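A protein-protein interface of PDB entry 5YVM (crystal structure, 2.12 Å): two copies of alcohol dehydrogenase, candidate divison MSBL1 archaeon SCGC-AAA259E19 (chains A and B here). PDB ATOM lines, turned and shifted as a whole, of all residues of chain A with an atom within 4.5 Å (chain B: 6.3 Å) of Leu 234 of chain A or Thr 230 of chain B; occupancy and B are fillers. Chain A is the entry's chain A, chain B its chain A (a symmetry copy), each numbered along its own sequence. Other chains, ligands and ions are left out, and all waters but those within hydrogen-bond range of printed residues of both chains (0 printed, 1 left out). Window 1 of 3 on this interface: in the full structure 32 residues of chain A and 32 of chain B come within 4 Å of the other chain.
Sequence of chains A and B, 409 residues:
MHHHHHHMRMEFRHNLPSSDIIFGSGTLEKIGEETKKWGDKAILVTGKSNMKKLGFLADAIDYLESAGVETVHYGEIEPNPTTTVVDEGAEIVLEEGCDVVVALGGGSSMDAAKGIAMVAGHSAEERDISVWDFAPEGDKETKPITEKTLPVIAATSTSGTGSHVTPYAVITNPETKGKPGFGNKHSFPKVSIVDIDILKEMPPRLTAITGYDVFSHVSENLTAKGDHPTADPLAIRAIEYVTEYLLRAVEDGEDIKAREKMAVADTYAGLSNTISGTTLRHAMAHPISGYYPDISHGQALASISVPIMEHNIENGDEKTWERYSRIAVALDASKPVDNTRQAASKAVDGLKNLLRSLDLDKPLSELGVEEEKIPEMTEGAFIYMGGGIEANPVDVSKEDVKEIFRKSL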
ATOM      1  N   THR A 230      22.188 -14.373 -21.589  1.00  0.00           N
ATOM      2  CA  THR A 230      22.615 -15.766 -21.522  1.00  0.00           C
ATOM      3  C   THR A 230      22.553 -16.290 -20.095  1.00  0.00           C
ATOM      4  O   THR A 230      22.366 -17.501 -19.895  1.00  0.00           O
ATOM      5  CB  THR A 230      24.024 -15.920 -22.160  1.00  0.00           C
ATOM      6  OG1 THR A 230      24.954 -15.037 -21.547  1.00  0.00           O
ATOM      7  CG2 THR A 230      23.996 -15.528 -23.633  1.00  0.00           C
ATOM      8  N   ALA A 231      22.670 -15.407 -19.093  1.00  0.00           N
ATOM      9  CA  ALA A 231      22.534 -15.812 -17.700  1.00  0.00           C
ATOM     10  C   ALA A 231      21.072 -16.012 -17.307  1.00  0.00           C
ATOM     11  O   ALA A 231      20.774 -16.873 -16.470  1.00  0.00           O
ATOM     12  CB  ALA A 231      23.163 -14.755 -16.778  1.00  0.00           C
ATOM     13  N   ASP A 232      20.153 -15.251 -17.906  1.00  0.00           N
ATOM     14  CA  ASP A 232      18.806 -15.113 -17.345  1.00  0.00           C
ATOM     15  C   ASP A 232      18.006 -16.409 -17.269  1.00  0.00           C
ATOM     16  O   ASP A 232      17.406 -16.666 -16.212  1.00  0.00           O
ATOM     17  CB  ASP A 232      18.040 -14.022 -18.108  1.00  0.00           C
ATOM     18  CG  ASP A 232      18.671 -12.639 -17.899  1.00  0.00           C
ATOM     19  OD1 ASP A 232      19.531 -12.553 -16.981  1.00  0.00           O
ATOM     20  OD2 ASP A 232      18.333 -11.680 -18.662  1.00  0.00           O
ATOM     21  N   PRO A 233      17.922 -17.246 -18.306  1.00  0.00           N
ATOM     22  CA  PRO A 233      17.120 -18.476 -18.150  1.00  0.00           C
ATOM     23  C   PRO A 233      17.644 -19.380 -17.047  1.00  0.00           C
ATOM     24  O   PRO A 233      16.858 -20.048 -16.366  1.00  0.00           O
ATOM     25  CB  PRO A 233      17.223 -19.138 -19.529  1.00  0.00           C
ATOM     26  CG  PRO A 233      17.574 -18.006 -20.462  1.00  0.00           C
ATOM     27  CD  PRO A 233      18.477 -17.136 -19.661  1.00  0.00           C
ATOM     28  N   LEU A 234      18.959 -19.418 -16.858  1.00  0.00           N
ATOM     29  CA  LEU A 234      19.546 -20.199 -15.775  1.00  0.00           C
ATOM     30  C   LEU A 234      19.199 -19.599 -14.431  1.00  0.00           C
ATOM     31  O   LEU A 234      18.854 -20.327 -13.494  1.00  0.00           O
ATOM     32  CB  LEU A 234      21.070 -20.260 -15.951  1.00  0.00           C
ATOM     33  CG  LEU A 234      21.555 -20.683 -17.359  1.00  0.00           C
ATOM     34  CD1 LEU A 234      23.068 -20.721 -17.344  1.00  0.00           C
ATOM     35  CD2 LEU A 234      21.050 -22.082 -17.714  1.00  0.00           C
ATOM     36  N   ALA A 235      19.292 -18.270 -14.327  1.00  0.00           N
ATOM     37  CA  ALA A 235      18.985 -17.583 -13.078  1.00  0.00           C
ATOM     38  C   ALA A 235      17.524 -17.780 -12.686  1.00  0.00           C
ATOM     39  O   ALA A 235      17.199 -18.006 -11.508  1.00  0.00           O
ATOM     40  CB  ALA A 235      19.321 -16.093 -13.232  1.00  0.00           C
ATOM     41  N   ILE A 236      16.626 -17.712 -13.664  1.00  0.00           N
ATOM     42  CA  ILE A 236      15.200 -17.903 -13.394  1.00  0.00           C
ATOM     43  C   ILE A 236      14.925 -19.334 -12.961  1.00  0.00           C
ATOM     44  O   ILE A 236      14.212 -19.580 -11.978  1.00  0.00           O
ATOM     45  CB  ILE A 236      14.372 -17.537 -14.643  1.00  0.00           C
ATOM     46  CG1 ILE A 236      14.414 -16.033 -14.898  1.00  0.00           C
ATOM     47  CG2 ILE A 236      12.937 -18.023 -14.504  1.00  0.00           C
ATOM     48  CD1 ILE A 236      13.565 -15.267 -13.932  1.00  0.00           C
ATOM     49  N   ARG A 237      15.431 -20.302 -13.733  1.00  0.00           N
ATOM     50  CA  ARG A 237      15.235 -21.703 -13.385  1.00  0.00           C
ATOM     51  C   ARG A 237      15.761 -21.992 -11.982  1.00  0.00           C
ATOM     52  O   ARG A 237      15.169 -22.792 -11.243  1.00  0.00           O
ATOM     53  CB  ARG A 237      15.929 -22.596 -14.418  1.00  0.00           C
ATOM     54  CG  ARG A 237      15.518 -24.050 -14.367  1.00  0.00           C
ATOM     55  CD  ARG A 237      14.029 -24.181 -14.591  1.00  0.00           C
ATOM     56  NE  ARG A 237      13.607 -25.558 -14.813  1.00  0.00           N
ATOM     57  CZ  ARG A 237      12.332 -25.930 -14.824  1.00  0.00           C
ATOM     58  NH1 ARG A 237      11.987 -27.203 -15.029  1.00  0.00           N
ATOM     59  NH2 ARG A 237      11.394 -25.015 -14.612  1.00  0.00           N
ATOM     60  N   ALA A 238      16.859 -21.335 -11.590  1.00  0.00           N
ATOM     61  CA  ALA A 238      17.412 -21.561 -10.257  1.00  0.00           C
ATOM     62  C   ALA A 238      16.442 -21.090  -9.180  1.00  0.00           C
ATOM     63  O   ALA A 238      16.219 -21.797  -8.188  1.00  0.00           O
ATOM     64  CB  ALA A 238      18.762 -20.856 -10.106  1.00  0.00           C
ATOM     65  N   THR A 267      24.559 -25.036  -9.626  1.00  0.00           N
ATOM     66  CA  THR A 267      25.374 -24.990 -10.838  1.00  0.00           C
ATOM     67  C   THR A 267      24.880 -23.903 -11.791  1.00  0.00           C
ATOM     68  O   THR A 267      25.691 -23.155 -12.349  1.00  0.00           O
ATOM     69  CB  THR A 267      25.391 -26.378 -11.479  1.00  0.00           C
ATOM     70  OG1 THR A 267      26.044 -27.286 -10.572  1.00  0.00           O
ATOM     71  CG2 THR A 267      26.140 -26.369 -12.812  1.00  0.00           C
ATOM     72  N   TYR A 268      23.552 -23.728 -11.918  1.00  0.00           N
ATOM     73  CA  TYR A 268      23.043 -22.597 -12.696  1.00  0.00           C
ATOM     74  C   TYR A 268      23.593 -21.285 -12.152  1.00  0.00           C
ATOM     75  O   TYR A 268      24.009 -20.406 -12.923  1.00  0.00           O
ATOM     76  CB  TYR A 268      21.520 -22.535 -12.667  1.00  0.00           C
ATOM     77  CG  TYR A 268      20.753 -23.585 -13.436  1.00  0.00           C
ATOM     78  CD1 TYR A 268      21.335 -24.315 -14.462  1.00  0.00           C
ATOM     79  CD2 TYR A 268      19.418 -23.831 -13.133  1.00  0.00           C
ATOM     80  CE1 TYR A 268      20.598 -25.274 -15.146  1.00  0.00           C
ATOM     81  CE2 TYR A 268      18.678 -24.785 -13.816  1.00  0.00           C
ATOM     82  CZ  TYR A 268      19.271 -25.495 -14.830  1.00  0.00           C
ATOM     83  OH  TYR A 268      18.554 -26.462 -15.505  1.00  0.00           O
ATOM     84  N   LEU A 271      27.309 -20.548 -13.135  1.00  0.00           N
ATOM     85  CA  LEU A 271      27.364 -20.147 -14.535  1.00  0.00           C
ATOM     86  C   LEU A 271      26.797 -18.745 -14.715  1.00  0.00           C
ATOM     87  O   LEU A 271      27.382 -17.892 -15.415  1.00  0.00           O
ATOM     88  CB  LEU A 271      26.590 -21.159 -15.384  1.00  0.00           C
ATOM     89  CG  LEU A 271      27.178 -22.581 -15.367  1.00  0.00           C
ATOM     90  CD1 LEU A 271      26.319 -23.564 -16.180  1.00  0.00           C
ATOM     91  CD2 LEU A 271      28.621 -22.586 -15.887  1.00  0.00           C
ATOM     92  N   PHE B  12      24.881 -36.700 -15.390  1.00  0.00           N
ATOM     93  CA  PHE B  12      25.256 -36.125 -16.673  1.00  0.00           C
ATOM     94  C   PHE B  12      26.681 -35.596 -16.603  1.00  0.00           C
ATOM     95  O   PHE B  12      27.246 -35.386 -15.528  1.00  0.00           O
ATOM     96  CB  PHE B  12      24.282 -35.015 -17.113  1.00  0.00           C
ATOM     97  CG  PHE B  12      24.277 -33.803 -16.213  1.00  0.00           C
ATOM     98  CD1 PHE B  12      23.465 -33.769 -15.089  1.00  0.00           C
ATOM     99  CD2 PHE B  12      25.065 -32.690 -16.509  1.00  0.00           C
ATOM    100  CE1 PHE B  12      23.440 -32.660 -14.279  1.00  0.00           C
ATOM    101  CE2 PHE B  12      25.062 -31.578 -15.696  1.00  0.00           C
ATOM    102  CZ  PHE B  12      24.248 -31.560 -14.582  1.00  0.00           C
ATOM    103  N   HIS B  14      28.453 -32.291 -18.376  1.00  0.00           N
ATOM    104  CA  HIS B  14      28.295 -31.063 -19.138  1.00  0.00           C
ATOM    105  C   HIS B  14      29.668 -30.631 -19.649  1.00  0.00           C
ATOM    106  O   HIS B  14      30.616 -30.531 -18.872  1.00  0.00           O
ATOM    107  CB  HIS B  14      27.667 -30.017 -18.228  1.00  0.00           C
ATOM    108  CG  HIS B  14      27.737 -28.615 -18.733  1.00  0.00           C
ATOM    109  ND1 HIS B  14      26.663 -27.990 -19.323  1.00  0.00           N
ATOM    110  CD2 HIS B  14      28.729 -27.694 -18.675  1.00  0.00           C
ATOM    111  CE1 HIS B  14      27.000 -26.753 -19.644  1.00  0.00           C
ATOM    112  NE2 HIS B  14      28.242 -26.544 -19.246  1.00  0.00           N
ATOM    113  N   ASN B  15      29.775 -30.409 -20.957  1.00  0.00           N
ATOM    114  CA  ASN B  15      31.007 -29.921 -21.551  1.00  0.00           C
ATOM    115  C   ASN B  15      30.668 -28.749 -22.449  1.00  0.00           C
ATOM    116  O   ASN B  15      29.891 -28.890 -23.407  1.00  0.00           O
ATOM    117  CB  ASN B  15      31.725 -31.025 -22.329  1.00  0.00           C
ATOM    118  CG  ASN B  15      32.307 -32.092 -21.409  1.00  0.00           C
ATOM    119  OD1 ASN B  15      31.866 -33.248 -21.421  1.00  0.00           O
ATOM    120  ND2 ASN B  15      33.303 -31.714 -20.606  1.00  0.00           N
ATOM    121  N   HIS B 228      20.199 -33.353 -19.244  1.00  0.00           N
ATOM    122  CA  HIS B 228      21.054 -32.267 -19.715  1.00  0.00           C
ATOM    123  C   HIS B 228      20.525 -30.945 -19.173  1.00  0.00           C
ATOM    124  O   HIS B 228      20.172 -30.043 -19.936  1.00  0.00           O
ATOM    125  CB  HIS B 228      21.123 -32.263 -21.250  1.00  0.00           C
ATOM    126  CG  HIS B 228      19.925 -32.888 -21.910  1.00  0.00           C
ATOM    127  ND1 HIS B 228      18.702 -32.254 -21.989  1.00  0.00           N
ATOM    128  CD2 HIS B 228      19.757 -34.095 -22.502  1.00  0.00           C
ATOM    129  CE1 HIS B 228      17.836 -33.040 -22.606  1.00  0.00           C
ATOM    130  NE2 HIS B 228      18.454 -34.159 -22.939  1.00  0.00           N
ATOM    131  N   PRO B 229      20.500 -30.786 -17.836  1.00  0.00           N
ATOM    132  CA  PRO B 229      19.806 -29.622 -17.242  1.00  0.00           C
ATOM    133  C   PRO B 229      20.424 -28.277 -17.590  1.00  0.00           C
ATOM    134  O   PRO B 229      19.727 -27.251 -17.513  1.00  0.00           O
ATOM    135  CB  PRO B 229      19.897 -29.882 -15.728  1.00  0.00           C
ATOM    136  CG  PRO B 229      20.308 -31.314 -15.590  1.00  0.00           C
ATOM    137  CD  PRO B 229      21.108 -31.645 -16.801  1.00  0.00           C
ATOM    138  N   THR B 230      21.708 -28.226 -17.945  1.00  0.00           N
ATOM    139  CA  THR B 230      22.298 -26.915 -18.185  1.00  0.00           C
ATOM    140  C   THR B 230      21.851 -26.350 -19.526  1.00  0.00           C
ATOM    141  O   THR B 230      21.797 -25.119 -19.685  1.00  0.00           O
ATOM    142  CB  THR B 230      23.844 -26.994 -18.050  1.00  0.00           C
ATOM    143  OG1 THR B 230      24.374 -27.994 -18.911  1.00  0.00           O
ATOM    144  CG2 THR B 230      24.241 -27.417 -16.640  1.00  0.00           C
ATOM    145  N   ALA B 231      21.496 -27.215 -20.487  1.00  0.00           N
ATOM    146  CA  ALA B 231      20.973 -26.757 -21.769  1.00  0.00           C
ATOM    147  C   ALA B 231      19.512 -26.325 -21.664  1.00  0.00           C
ATOM    148  O   ALA B 231      19.091 -25.407 -22.378  1.00  0.00           O
ATOM    149  CB  ALA B 231      21.094 -27.873 -22.818  1.00  0.00           C
ATOM    150  N   ASP B 232      18.736 -26.951 -20.777  1.00  0.00           N
ATOM    151  CA  ASP B 232      17.275 -26.866 -20.860  1.00  0.00           C
ATOM    152  C   ASP B 232      16.703 -25.461 -20.703  1.00  0.00           C
ATOM    153  O   ASP B 232      15.837 -25.088 -21.510  1.00  0.00           O
ATOM    154  CB  ASP B 232      16.644 -27.846 -19.859  1.00  0.00           C
ATOM    155  CG  ASP B 232      16.952 -29.304 -20.228  1.00  0.00           C
ATOM    156  OD1 ASP B 232      17.439 -29.496 -21.375  1.00  0.00           O
ATOM    157  OD2 ASP B 232      16.740 -30.219 -19.372  1.00  0.00           O
ATOM    158  N   PRO B 233      17.094 -24.649 -19.718  1.00  0.00           N
ATOM    159  CA  PRO B 233      16.484 -23.306 -19.633  1.00  0.00           C
ATOM    160  C   PRO B 233      16.749 -22.465 -20.871  1.00  0.00           C
ATOM    161  O   PRO B 233      15.895 -21.667 -21.273  1.00  0.00           O
ATOM    162  CB  PRO B 233      17.135 -22.704 -18.383  1.00  0.00           C
ATOM    163  CG  PRO B 233      17.595 -23.901 -17.588  1.00  0.00           C
ATOM    164  CD  PRO B 233      18.039 -24.878 -18.618  1.00  0.00           C
ATOM    165  N   LEU B 234      17.918 -22.624 -21.482  1.00  0.00           N
ATOM    166  CA  LEU B 234      18.228 -21.915 -22.718  1.00  0.00           C
ATOM    167  C   LEU B 234      17.372 -22.419 -23.857  1.00  0.00           C
ATOM    168  O   LEU B 234      16.854 -21.623 -24.647  1.00  0.00           O
ATOM    169  CB  LEU B 234      19.716 -22.093 -23.054  1.00  0.00           C
ATOM    170  CG  LEU B 234      20.695 -21.786 -21.896  1.00  0.00           C
ATOM    171  CD1 LEU B 234      22.107 -21.981 -22.408  1.00  0.00           C
ATOM    172  CD2 LEU B 234      20.557 -20.336 -21.431  1.00  0.00           C
ATOM    173  N   ILE B 275      25.985 -28.339 -25.510  1.00  0.00           N
ATOM    174  CA  ILE B 275      25.840 -29.111 -24.272  1.00  0.00           C
ATOM    175  C   ILE B 275      25.088 -30.408 -24.531  1.00  0.00           C
ATOM    176  O   ILE B 275      25.499 -31.490 -24.094  1.00  0.00           O
ATOM    177  CB  ILE B 275      25.111 -28.287 -23.196  1.00  0.00           C
ATOM    178  CG1 ILE B 275      25.945 -27.094 -22.725  1.00  0.00           C
ATOM    179  CG2 ILE B 275      24.754 -29.183 -22.021  1.00  0.00           C
ATOM    180  CD1 ILE B 275      25.093 -25.997 -22.167  1.00  0.00           C
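OH of Tyr 268 of chain A is in hydrogen-bond range of O of Pro 229 of chain B (2.5 Å).
Among the printed residues, merely in contact across the chains: Pro 233 of chain A with Pro 233 of chain B, Tyr 268 of chain A with Pro 233 of chain B, Leu 234 of chain A with Thr 230 of chain B, Thr 230 of chain A with Leu 234 of chain B, Arg 237 of chain A with Pro 233 of chain B, Tyr 268 of chain A with Thr 230 of chain B, Leu 234 of chain A with Pro 233 of chain B and Pro 233 of chain A with Leu 234 of chain B.
Of the printed residues of chain B, Thr 230 of chain A touches Leu 234 (3.7 Å).
Printed residues of chain B within 4 Å of Pro 233 of chain A: Pro 233 and Leu 234.
Thr 267 of chain A touches none of the printed residues of chain B.
Of the printed residues of chain B, Tyr 268 of chain A touches Pro 229, Thr 230 and Pro 233.
His 14 of chain B touches none of the printed residues of chain A.
Of the printed residues of chain A, Pro 229 of chain B touches Tyr 268.
Printed residues of chain A within 4 Å of Pro 233 of chain B: Pro 233 (3.3 Å), Leu 234 (3.9 Å), Arg 237 (3.8 Å) and Tyr 268 (3.4 Å).
Printed residues of chain A that touch a printed residue of chain B: Thr 230, Pro 233, Leu 234, Arg 237 and Tyr 268.
Among the printed residues, no Asp or Glu carboxylate lies within 4 Å of a Lys or Arg side-chain nitrogen of the other chain.
Thr 230 of chain A touches Leu 234 of chain B, and with the chains exchanged Leu 234 of chain A touches Thr 230 of chain B.
Pro 233 of chain B touches its own counterpart, Pro 233 of chain A.
Pro 233 of chain A touches Leu 234 of chain B, and with the chains exchanged Leu 234 of chain A touches Pro 233 of chain B.
Positions printed for both chains: 230, 231, 232, 233 and 234.
Of the 9 pairs that touch across the chains among the printed residues, 5 have their exchanged pair printed and touching as well.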
